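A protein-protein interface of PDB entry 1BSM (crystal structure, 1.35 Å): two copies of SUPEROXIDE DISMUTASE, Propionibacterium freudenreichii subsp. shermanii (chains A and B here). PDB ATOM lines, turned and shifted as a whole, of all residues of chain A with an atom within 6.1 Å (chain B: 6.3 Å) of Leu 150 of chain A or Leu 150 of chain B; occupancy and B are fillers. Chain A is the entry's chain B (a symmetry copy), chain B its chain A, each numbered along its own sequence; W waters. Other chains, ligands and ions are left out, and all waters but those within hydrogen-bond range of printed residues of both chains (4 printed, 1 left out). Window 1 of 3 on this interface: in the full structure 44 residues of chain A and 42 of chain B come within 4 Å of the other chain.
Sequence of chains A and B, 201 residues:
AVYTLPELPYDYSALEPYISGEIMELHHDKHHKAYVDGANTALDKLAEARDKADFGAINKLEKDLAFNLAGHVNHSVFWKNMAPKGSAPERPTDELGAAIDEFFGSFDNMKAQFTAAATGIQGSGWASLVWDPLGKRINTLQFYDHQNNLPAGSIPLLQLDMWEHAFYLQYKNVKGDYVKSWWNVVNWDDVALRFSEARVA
O of Gln 147 of chain B is in hydrogen-bond range of N of Asn 149 of chain A, 2.9 Å away.
O of Gln 147 of chain B is in hydrogen-bond range of N of Leu 150 of chain A (3.0 Å).
The side-chain amide oxygen of Asn 148 of chain B is in hydrogen-bond range of the backbone NH of Asn 149 of chain A, 3.0 Å away.
O of Gln 147 of chain A is in hydrogen-bond range of N of Asn 149 of chain B.
The backbone NH (N) of Asn 149 of chain B is in hydrogen-bond range of the side-chain amide oxygen (OD1) of Asn 148 of chain A (2.9 Å).
The backbone NH (N) of Leu 150 of chain B is in hydrogen-bond range of the backbone carbonyl oxygen (O) of Gln 147 of chain A.
N of Gly 153 of chain B lies within hydrogen-bond range of O of Ser 154 of chain A (2.7 Å).
O of Ser 154 of chain B sits at hydrogen-bond distance from N of Gly 153 of chain A (2.6 Å).
ND2 of Asn 74 of chain B sits close to O of Ala 70 of chain B (3.1 Å).
The backbone carbonyl oxygen of Gln 142 of chain B sits close to the side-chain amide oxygen of Asn 149 of chain B (2.7 Å).
The backbone carbonyl oxygen (O) of Pro 151 of chain B sits at hydrogen-bond distance from the side-chain hydroxyl (OG) of Ser 154 of chain B (2.7 Å).
The backbone carbonyl oxygen (O) of Gln 142 of chain A sits close to the side-chain amide oxygen (OD1) of Asn 149 of chain A (2.8 Å).
OE1 of Gln 147 of chain A lies within hydrogen-bond range of ND2 of Asn 148 of chain A (3.5 Å).
The side-chain hydroxyl of Ser 154 of chain A lies within hydrogen-bond range of the backbone carbonyl oxygen of Pro 151 of chain A.
Among the printed residues, merely in contact across the chains: Ala 66 of chain A with Asn 149 of chain B (3.4 Å), Ala 66 of chain A with Leu 150 of chain B (3.9 Å), Ala 66 of chain A with Pro 151 of chain B (3.9 Å), Ala 70 of chain A with Pro 151 of chain B (3.7 Å), Gln 147 of chain A with Asn 148 of chain B (3.8 Å), Asn 148 of chain A with Gln 147 of chain B (3.8 Å), Asn 148 of chain A with Asn 148 of chain B (3.4 Å), Asn 149 of chain A with Ala 66 of chain B (3.4 Å), Leu 150 of chain A with Ala 66 of chain B (3.9 Å), Leu 150 of chain A with Leu 150 of chain B (3.5 Å), Leu 150 of chain A with Ala 152 of chain B (3.5 Å), Pro 151 of chain A with Ala 66 of chain B (3.9 Å), Pro 151 of chain A with Ala 70 of chain B (3.8 Å), Ala 152 of chain A with Leu 150 of chain B (3.4 Å), Ala 152 of chain A with Ser 154 of chain B (3.7 Å) and Ser 154 of chain A with Ala 152 of chain B (3.7 Å).
Leu 150 of chain A touches just these residues of chain B: Ala 66 (3.9 Å), Gln 147 (3.0 Å), Leu 150 (3.5 Å) and Ala 152 (3.5 Å).
Leu 150 of chain B touches just these residues of chain A: Ala 66, Gln 147, Leu 150 and Ala 152.
Printed residues of chain A within 4 Å of Asn 148 of chain B: Gln 147, Asn 148 and Asn 149.
Of the printed residues of chain B, Ala 66 of chain A touches Asn 149, Leu 150 and Pro 151.
Printed residues of chain A within 4 Å of Gln 147 of chain B: Asn 148, Asn 149 and Leu 150.
Of the printed residues of chain A, Gly 153 of chain B touches Ser 154.
Of the printed residues of chain B, Asn 148 of chain A touches Gln 147, Asn 148 and Asn 149.
The nearest residue of chain A that does not touch Leu 150 of chain B is Pro 151 of chain A (4.2 Å).
Hydrophobic or aromatic side chains of chain B that line the printed part of chain A: Ala 66, Ala 70, Leu 150, Pro 151 and Ala 152.
Along chain B the printed residues that touch a printed residue of chain A span positions 66 to 154.
Of the 14 printed residues of chain A, 10 touch a printed residue of chain B.
Hydrophobic or aromatic side chains of chain A within 4 Å of the printed part of chain B: Ala 66, Ala 70, Leu 150, Pro 151 and Ala 152.
Among the printed residues, 24 pairs touch across the chains.
Among the printed residues, no Asp or Glu carboxylate lies within 4 Å of a Lys or Arg side-chain nitrogen of the other chain.
Ala 66 of chain A touches Asn 149 of chain B, and with the chains exchanged Asn 149 of chain A touches Ala 66 of chain B.
Gln 147 of chain A touches Asn 148 of chain B, and with the chains exchanged Asn 148 of chain A touches Gln 147 of chain B.
Gln 147 of chain A touches Leu 150 of chain B, and with the chains exchanged Leu 150 of chain A touches Gln 147 of chain B.
Gly 153 of chain A touches Ser 154 of chain B, and with the chains exchanged Ser 154 of chain A touches Gly 153 of chain B.
Positions printed for both chains: 66, 70, 141, 142, 143, 146, 147, 148, 149, 150, 151, 152, 153 and 154.
Of the 24 pairs that touch across the chains among the printed residues, 24 have their exchanged pair printed and touching as well.
Water W3 lies within hydrogen-bond range of the side-chain amide oxygen of Gln 147 of chain A (2.7 Å), the side-chain amide nitrogen of Asn 149 of chain B (2.8 Å) and the side-chain amide oxygen of Asn 148 of chain A (2.8 Å).
Water W2 bridges the backbone NH of Ala 152 of chain B (2.7 Å) and the backbone carbonyl oxygen of His 146 of chain A (3.0 Å).
Water W1 lies within hydrogen-bond range of the side-chain amide nitrogen of Asn 149 of chain A (2.8 Å), the side-chain amide oxygen of Asn 148 of chain B (2.8 Å) and the side-chain amide oxygen of Gln 147 of chain B (2.8 Å).
Water W4 lies within hydrogen-bond range of the side-chain amide oxygen (OD1) of Asn 74 of chain B (2.8 Å), the backbone NH (N) of Ala 152 of chain A (2.8 Å) and the backbone carbonyl oxygen (O) of His 146 of chain B (2.9 Å).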
ATOM      1  N   ALA A  66      22.456 -14.686  -2.328  1.00  0.00           N
ATOM      2  CA  ALA A  66      22.084 -15.562  -1.222  1.00  0.00           C
ATOM      3  C   ALA A  66      23.237 -16.463  -0.781  1.00  0.00           C
ATOM      4  O   ALA A  66      23.532 -16.555   0.404  1.00  0.00           O
ATOM      5  CB  ALA A  66      20.863 -16.399  -1.592  1.00  0.00           C
ATOM      6  N   ALA A  70      25.086 -15.357   2.573  1.00  0.00           N
ATOM      7  CA  ALA A  70      24.855 -16.359   3.612  1.00  0.00           C
ATOM      8  C   ALA A  70      26.198 -16.921   4.075  1.00  0.00           C
ATOM      9  O   ALA A  70      26.376 -17.223   5.251  1.00  0.00           O
ATOM     10  CB  ALA A  70      23.967 -17.476   3.099  1.00  0.00           C
ATOM     11  N   LEU A 141      18.674 -26.019  13.332  1.00  0.00           N
ATOM     12  CA  LEU A 141      18.415 -26.112  11.903  1.00  0.00           C
ATOM     13  C   LEU A 141      19.638 -26.729  11.240  1.00  0.00           C
ATOM     14  O   LEU A 141      20.754 -26.644  11.762  1.00  0.00           O
ATOM     15  CB  LEU A 141      18.151 -24.729  11.299  1.00  0.00           C
ATOM     16  CG  LEU A 141      16.877 -23.979  11.704  1.00  0.00           C
ATOM     17  CD1 LEU A 141      16.891 -22.582  11.101  1.00  0.00           C
ATOM     18  CD2 LEU A 141      15.643 -24.746  11.243  1.00  0.00           C
ATOM     19  N   GLN A 142      19.412 -27.378  10.105  1.00  0.00           N
ATOM     20  CA  GLN A 142      20.483 -28.000   9.350  1.00  0.00           C
ATOM     21  C   GLN A 142      20.529 -27.298   7.999  1.00  0.00           C
ATOM     22  O   GLN A 142      19.722 -27.591   7.117  1.00  0.00           O
ATOM     23  CB  GLN A 142      20.199 -29.491   9.165  1.00  0.00           C
ATOM     24  CG  GLN A 142      21.335 -30.272   8.525  1.00  0.00           C
ATOM     25  CD  GLN A 142      20.923 -31.681   8.140  1.00  0.00           C
ATOM     26  OE1 GLN A 142      20.242 -31.881   7.136  1.00  0.00           O
ATOM     27  NE2 GLN A 142      21.321 -32.663   8.943  1.00  0.00           N
ATOM     28  N   PHE A 143      21.432 -26.330   7.860  1.00  0.00           N
ATOM     29  CA  PHE A 143      21.562 -25.592   6.608  1.00  0.00           C
ATOM     30  C   PHE A 143      22.204 -26.472   5.545  1.00  0.00           C
ATOM     31  O   PHE A 143      23.010 -27.346   5.863  1.00  0.00           O
ATOM     32  CB  PHE A 143      22.478 -24.370   6.760  1.00  0.00           C
ATOM     33  CG  PHE A 143      21.996 -23.331   7.738  1.00  0.00           C
ATOM     34  CD1 PHE A 143      20.757 -23.433   8.363  1.00  0.00           C
ATOM     35  CD2 PHE A 143      22.807 -22.237   8.029  1.00  0.00           C
ATOM     36  CE1 PHE A 143      20.331 -22.449   9.255  1.00  0.00           C
ATOM     37  CE2 PHE A 143      22.388 -21.249   8.917  1.00  0.00           C
ATOM     38  CZ  PHE A 143      21.152 -21.356   9.535  1.00  0.00           C
ATOM     39  N   HIS A 146      25.007 -22.878   2.305  1.00  0.00           N
ATOM     40  CA  HIS A 146      25.024 -21.736   3.223  1.00  0.00           C
ATOM     41  C   HIS A 146      23.657 -21.083   3.359  1.00  0.00           C
ATOM     42  O   HIS A 146      23.285 -20.605   4.433  1.00  0.00           O
ATOM     43  CB  HIS A 146      25.967 -20.642   2.718  1.00  0.00           C
ATOM     44  CG  HIS A 146      27.414 -21.002   2.793  1.00  0.00           C
ATOM     45  ND1 HIS A 146      28.270 -20.859   1.725  1.00  0.00           N
ATOM     46  CD2 HIS A 146      28.157 -21.498   3.809  1.00  0.00           C
ATOM     47  CE1 HIS A 146      29.477 -21.256   2.079  1.00  0.00           C
ATOM     48  NE2 HIS A 146      29.435 -21.647   3.338  1.00  0.00           N
ATOM     49  N   GLN A 147      22.905 -21.130   2.264  1.00  0.00           N
ATOM     50  CA  GLN A 147      21.623 -20.458   2.151  1.00  0.00           C
ATOM     51  C   GLN A 147      20.355 -21.298   2.017  1.00  0.00           C
ATOM     52  O   GLN A 147      19.287 -20.752   1.729  1.00  0.00           O
ATOM     53  CB  GLN A 147      21.721 -19.477   0.970  1.00  0.00           C
ATOM     54  CG  GLN A 147      21.587 -20.090  -0.449  1.00  0.00           C
ATOM     55  CD  GLN A 147      22.719 -21.032  -0.903  1.00  0.00           C
ATOM     56  OE1 GLN A 147      22.599 -21.676  -1.947  1.00  0.00           O
ATOM     57  NE2 GLN A 147      23.816 -21.086  -0.159  1.00  0.00           N
ATOM     58  N   ASN A 148      20.447 -22.599   2.261  1.00  0.00           N
ATOM     59  CA  ASN A 148      19.275 -23.464   2.125  1.00  0.00           C
ATOM     60  C   ASN A 148      18.851 -24.167   3.410  1.00  0.00           C
ATOM     61  O   ASN A 148      19.659 -24.370   4.321  1.00  0.00           O
ATOM     62  CB  ASN A 148      19.512 -24.502   1.023  1.00  0.00           C
ATOM     63  CG  ASN A 148      19.835 -23.870  -0.320  1.00  0.00           C
ATOM     64  OD1 ASN A 148      19.250 -22.850  -0.701  1.00  0.00           O
ATOM     65  ND2 ASN A 148      20.775 -24.471  -1.044  1.00  0.00           N
ATOM     66  N   ASN A 149      17.570 -24.523   3.463  1.00  0.00           N
ATOM     67  CA  ASN A 149      16.959 -25.232   4.588  1.00  0.00           C
ATOM     68  C   ASN A 149      16.811 -24.409   5.875  1.00  0.00           C
ATOM     69  O   ASN A 149      17.141 -24.882   6.962  1.00  0.00           O
ATOM     70  CB  ASN A 149      17.720 -26.541   4.856  1.00  0.00           C
ATOM     71  CG  ASN A 149      16.818 -27.666   5.351  1.00  0.00           C
ATOM     72  OD1 ASN A 149      17.209 -28.452   6.215  1.00  0.00           O
ATOM     73  ND2 ASN A 149      15.624 -27.772   4.776  1.00  0.00           N
ATOM     74  N   LEU A 150      16.282 -23.190   5.748  1.00  0.00           N
ATOM     75  CA  LEU A 150      16.077 -22.309   6.901  1.00  0.00           C
ATOM     76  C   LEU A 150      14.984 -21.269   6.642  1.00  0.00           C
ATOM     77  O   LEU A 150      14.846 -20.771   5.523  1.00  0.00           O
ATOM     78  CB  LEU A 150      17.378 -21.582   7.284  1.00  0.00           C
ATOM     79  CG  LEU A 150      17.884 -20.443   6.388  1.00  0.00           C
ATOM     80  CD1 LEU A 150      18.891 -19.590   7.142  1.00  0.00           C
ATOM     81  CD2 LEU A 150      18.486 -20.990   5.113  1.00  0.00           C
ATOM     82  N   PRO A 151      14.175 -20.957   7.667  1.00  0.00           N
ATOM     83  CA  PRO A 151      13.104 -19.966   7.516  1.00  0.00           C
ATOM     84  C   PRO A 151      13.658 -18.545   7.541  1.00  0.00           C
ATOM     85  O   PRO A 151      14.680 -18.276   8.182  1.00  0.00           O
ATOM     86  CB  PRO A 151      12.232 -20.201   8.756  1.00  0.00           C
ATOM     87  CG  PRO A 151      12.533 -21.614   9.149  1.00  0.00           C
ATOM     88  CD  PRO A 151      14.021 -21.688   8.936  1.00  0.00           C
ATOM     89  N   ALA A 152      12.985 -17.639   6.838  1.00  0.00           N
ATOM     90  CA  ALA A 152      13.394 -16.240   6.823  1.00  0.00           C
ATOM     91  C   ALA A 152      13.193 -15.722   8.246  1.00  0.00           C
ATOM     92  O   ALA A 152      12.282 -16.167   8.947  1.00  0.00           O
ATOM     93  CB  ALA A 152      12.530 -15.448   5.852  1.00  0.00           C
ATOM     94  N   GLY A 153      14.072 -14.826   8.684  1.00  0.00           N
ATOM     95  CA  GLY A 153      13.955 -14.277  10.024  1.00  0.00           C
ATOM     96  C   GLY A 153      14.664 -15.056  11.120  1.00  0.00           C
ATOM     97  O   GLY A 153      14.643 -14.646  12.279  1.00  0.00           O
ATOM     98  N   SER A 154      15.271 -16.191  10.770  1.00  0.00           N
ATOM     99  CA  SER A 154      15.997 -17.001  11.745  1.00  0.00           C
ATOM    100  C   SER A 154      17.246 -16.244  12.200  1.00  0.00           C
ATOM    101  O   SER A 154      18.024 -15.768  11.371  1.00  0.00           O
ATOM    102  CB  SER A 154      16.419 -18.338  11.126  1.00  0.00           C
ATOM    103  OG  SER A 154      15.300 -19.069  10.657  1.00  0.00           O
ATOM    104  N   ALA B  66      12.170 -26.778   8.705  1.00  0.00           N
ATOM    105  CA  ALA B  66      12.534 -25.647   7.858  1.00  0.00           C
ATOM    106  C   ALA B  66      11.463 -25.336   6.814  1.00  0.00           C
ATOM    107  O   ALA B  66      11.092 -24.182   6.627  1.00  0.00           O
ATOM    108  CB  ALA B  66      13.876 -25.903   7.179  1.00  0.00           C
ATOM    109  N   PHE B  67      10.962 -26.374   6.150  1.00  0.00           N
ATOM    110  CA  PHE B  67       9.937 -26.223   5.118  1.00  0.00           C
ATOM    111  C   PHE B  67       8.626 -25.683   5.685  1.00  0.00           C
ATOM    112  O   PHE B  67       8.093 -24.685   5.200  1.00  0.00           O
ATOM    113  CB  PHE B  67       9.689 -27.567   4.416  1.00  0.00           C
ATOM    114  CG  PHE B  67       8.553 -27.542   3.427  1.00  0.00           C
ATOM    115  CD1 PHE B  67       8.675 -26.856   2.221  1.00  0.00           C
ATOM    116  CD2 PHE B  67       7.359 -28.202   3.704  1.00  0.00           C
ATOM    117  CE1 PHE B  67       7.622 -26.823   1.307  1.00  0.00           C
ATOM    118  CE2 PHE B  67       6.302 -28.176   2.797  1.00  0.00           C
ATOM    119  CZ  PHE B  67       6.435 -27.486   1.597  1.00  0.00           C
ATOM    120  N   ALA B  70       9.074 -22.221   7.579  1.00  0.00           N
ATOM    121  CA  ALA B  70       9.296 -21.184   6.575  1.00  0.00           C
ATOM    122  C   ALA B  70       7.985 -20.859   5.863  1.00  0.00           C
ATOM    123  O   ALA B  70       7.741 -19.715   5.498  1.00  0.00           O
ATOM    124  CB  ALA B  70      10.342 -21.624   5.574  1.00  0.00           C
ATOM    125  N   ASN B  74       6.506 -17.201   6.001  1.00  0.00           N
ATOM    126  CA  ASN B  74       6.245 -16.542   4.724  1.00  0.00           C
ATOM    127  C   ASN B  74       4.790 -16.122   4.525  1.00  0.00           C
ATOM    128  O   ASN B  74       4.525 -15.005   4.082  1.00  0.00           O
ATOM    129  CB  ASN B  74       6.689 -17.432   3.559  1.00  0.00           C
ATOM    130  CG  ASN B  74       8.197 -17.611   3.496  1.00  0.00           C
ATOM    131  OD1 ASN B  74       8.948 -16.870   4.125  1.00  0.00           O
ATOM    132  ND2 ASN B  74       8.645 -18.592   2.719  1.00  0.00           N
ATOM    133  N   LEU B 141      15.427 -10.837  -2.525  1.00  0.00           N
ATOM    134  CA  LEU B 141      15.881 -12.217  -2.558  1.00  0.00           C
ATOM    135  C   LEU B 141      14.848 -13.040  -3.310  1.00  0.00           C
ATOM    136  O   LEU B 141      13.677 -12.666  -3.392  1.00  0.00           O
ATOM    137  CB  LEU B 141      16.035 -12.770  -1.139  1.00  0.00           C
ATOM    138  CG  LEU B 141      17.161 -12.224  -0.258  1.00  0.00           C
ATOM    139  CD1 LEU B 141      17.039 -12.807   1.142  1.00  0.00           C
ATOM    140  CD2 LEU B 141      18.520 -12.558  -0.863  1.00  0.00           C
ATOM    141  N   GLN B 142      15.293 -14.150  -3.884  1.00  0.00           N
ATOM    142  CA  GLN B 142      14.399 -15.036  -4.609  1.00  0.00           C
ATOM    143  C   GLN B 142      14.424 -16.380  -3.894  1.00  0.00           C
ATOM    144  O   GLN B 142      15.333 -17.182  -4.106  1.00  0.00           O
ATOM    145  CB  GLN B 142      14.857 -15.201  -6.059  1.00  0.00           C
ATOM    146  CG  GLN B 142      13.908 -16.022  -6.912  1.00  0.00           C
ATOM    147  CD  GLN B 142      14.495 -16.369  -8.267  1.00  0.00           C
ATOM    148  OE1 GLN B 142      15.395 -17.199  -8.369  1.00  0.00           O
ATOM    149  NE2 GLN B 142      13.989 -15.732  -9.316  1.00  0.00           N
ATOM    150  N   PHE B 143      13.446 -16.597  -3.016  1.00  0.00           N
ATOM    151  CA  PHE B 143      13.346 -17.842  -2.257  1.00  0.00           C
ATOM    152  C   PHE B 143      12.922 -18.989  -3.166  1.00  0.00           C
ATOM    153  O   PHE B 143      12.151 -18.787  -4.104  1.00  0.00           O
ATOM    154  CB  PHE B 143      12.263 -17.757  -1.168  1.00  0.00           C
ATOM    155  CG  PHE B 143      12.501 -16.716  -0.103  1.00  0.00           C
ATOM    156  CD1 PHE B 143      13.639 -15.912  -0.100  1.00  0.00           C
ATOM    157  CD2 PHE B 143      11.555 -16.542   0.907  1.00  0.00           C
ATOM    158  CE1 PHE B 143      13.830 -14.957   0.902  1.00  0.00           C
ATOM    159  CE2 PHE B 143      11.738 -15.593   1.909  1.00  0.00           C
ATOM    160  CZ  PHE B 143      12.876 -14.795   1.904  1.00  0.00           C
ATOM    161  N   HIS B 146      10.110 -22.517   0.204  1.00  0.00           N
ATOM    162  CA  HIS B 146       9.837 -21.587   1.303  1.00  0.00           C
ATOM    163  C   HIS B 146      11.100 -21.291   2.090  1.00  0.00           C
ATOM    164  O   HIS B 146      11.312 -20.168   2.552  1.00  0.00           O
ATOM    165  CB  HIS B 146       8.844 -22.183   2.306  1.00  0.00           C
ATOM    166  CG  HIS B 146       7.452 -22.329   1.786  1.00  0.00           C
ATOM    167  ND1 HIS B 146       6.730 -23.493   1.921  1.00  0.00           N
ATOM    168  CD2 HIS B 146       6.643 -21.452   1.147  1.00  0.00           C
ATOM    169  CE1 HIS B 146       5.533 -23.327   1.385  1.00  0.00           C
ATOM    170  NE2 HIS B 146       5.456 -22.100   0.909  1.00  0.00           N
ATOM    171  N   GLN B 147      11.959 -22.301   2.162  1.00  0.00           N
ATOM    172  CA  GLN B 147      13.166 -22.269   2.970  1.00  0.00           C
ATOM    173  C   GLN B 147      14.527 -22.258   2.277  1.00  0.00           C
ATOM    174  O   GLN B 147      15.550 -22.439   2.943  1.00  0.00           O
ATOM    175  CB  GLN B 147      13.106 -23.464   3.930  1.00  0.00           C
ATOM    176  CG  GLN B 147      13.462 -24.842   3.315  1.00  0.00           C
ATOM    177  CD  GLN B 147      12.416 -25.465   2.365  1.00  0.00           C
ATOM    178  OE1 GLN B 147      12.634 -26.563   1.852  1.00  0.00           O
ATOM    179  NE2 GLN B 147      11.285 -24.798   2.158  1.00  0.00           N
ATOM    180  N   ASN B 148      14.559 -22.023   0.968  1.00  0.00           N
ATOM    181  CA  ASN B 148      15.829 -22.032   0.246  1.00  0.00           C
ATOM    182  C   ASN B 148      16.188 -20.717  -0.438  1.00  0.00           C
ATOM    183  O   ASN B 148      15.311 -19.919  -0.770  1.00  0.00           O
ATOM    184  CB  ASN B 148      15.840 -23.165  -0.789  1.00  0.00           C
ATOM    185  CG  ASN B 148      15.594 -24.528  -0.170  1.00  0.00           C
ATOM    186  OD1 ASN B 148      16.083 -24.825   0.919  1.00  0.00           O
ATOM    187  ND2 ASN B 148      14.830 -25.366  -0.865  1.00  0.00           N
ATOM    188  N   ASN B 149      17.489 -20.509  -0.631  1.00  0.00           N
ATOM    189  CA  ASN B 149      18.040 -19.326  -1.295  1.00  0.00           C
ATOM    190  C   ASN B 149      17.938 -18.024  -0.492  1.00  0.00           C
ATOM    191  O   ASN B 149      17.544 -16.987  -1.027  1.00  0.00           O
ATOM    192  CB  ASN B 149      17.413 -19.159  -2.691  1.00  0.00           C
ATOM    193  CG  ASN B 149      18.374 -18.550  -3.703  1.00  0.00           C
ATOM    194  OD1 ASN B 149      17.995 -17.691  -4.504  1.00  0.00           O
ATOM    195  ND2 ASN B 149      19.620 -19.014  -3.693  1.00  0.00           N
ATOM    196  N   LEU B 150      18.328 -18.075   0.782  1.00  0.00           N
ATOM    197  CA  LEU B 150      18.288 -16.894   1.642  1.00  0.00           C
ATOM    198  C   LEU B 150      19.273 -16.992   2.802  1.00  0.00           C
ATOM    199  O   LEU B 150      19.519 -18.080   3.329  1.00  0.00           O
ATOM    200  CB  LEU B 150      16.875 -16.670   2.205  1.00  0.00           C
ATOM    201  CG  LEU B 150      16.363 -17.602   3.310  1.00  0.00           C
ATOM    202  CD1 LEU B 150      15.137 -16.993   3.973  1.00  0.00           C
ATOM    203  CD2 LEU B 150      16.055 -18.979   2.762  1.00  0.00           C
ATOM    204  N   PRO B 151      19.889 -15.863   3.186  1.00  0.00           N
ATOM    205  CA  PRO B 151      20.850 -15.842   4.291  1.00  0.00           C
ATOM    206  C   PRO B 151      20.136 -15.885   5.644  1.00  0.00           C
ATOM    207  O   PRO B 151      18.994 -15.438   5.766  1.00  0.00           O
ATOM    208  CB  PRO B 151      21.548 -14.490   4.120  1.00  0.00           C
ATOM    209  CG  PRO B 151      21.370 -14.175   2.665  1.00  0.00           C
ATOM    210  CD  PRO B 151      19.953 -14.598   2.429  1.00  0.00           C
ATOM    211  N   ALA B 152      20.811 -16.425   6.651  1.00  0.00           N
ATOM    212  CA  ALA B 152      20.251 -16.476   7.996  1.00  0.00           C
ATOM    213  C   ALA B 152      20.222 -15.032   8.498  1.00  0.00           C
ATOM    214  O   ALA B 152      21.103 -14.246   8.159  1.00  0.00           O
ATOM    215  CB  ALA B 152      21.128 -17.332   8.900  1.00  0.00           C
ATOM    216  N   GLY B 153      19.188 -14.672   9.252  1.00  0.00           N
ATOM    217  CA  GLY B 153      19.089 -13.315   9.767  1.00  0.00           C
ATOM    218  C   GLY B 153      18.320 -12.351   8.877  1.00  0.00           C
ATOM    219  O   GLY B 153      18.092 -11.203   9.263  1.00  0.00           O
ATOM    220  N   SER B 154      17.937 -12.802   7.682  1.00  0.00           N
ATOM    221  CA  SER B 154      17.174 -11.972   6.750  1.00  0.00           C
ATOM    222  C   SER B 154      15.814 -11.663   7.362  1.00  0.00           C
ATOM    223  O   SER B 154      15.114 -12.569   7.814  1.00  0.00           O
ATOM    224  CB  SER B 154      16.958 -12.702   5.422  1.00  0.00           C
ATOM    225  OG  SER B 154      18.183 -13.011   4.786  1.00  0.00           O
HETATM  226  O   HOH W   1      15.380 -27.286   2.067  1.00  0.00           O
HETATM  227  O   HOH W   2      22.801 -18.283   6.307  1.00  0.00           O
HETATM  228  O   HOH W   3      20.147 -21.656  -3.049  1.00  0.00           O
HETATM  229  O   HOH W   4      11.252 -18.297   4.741  1.00  0.00           O
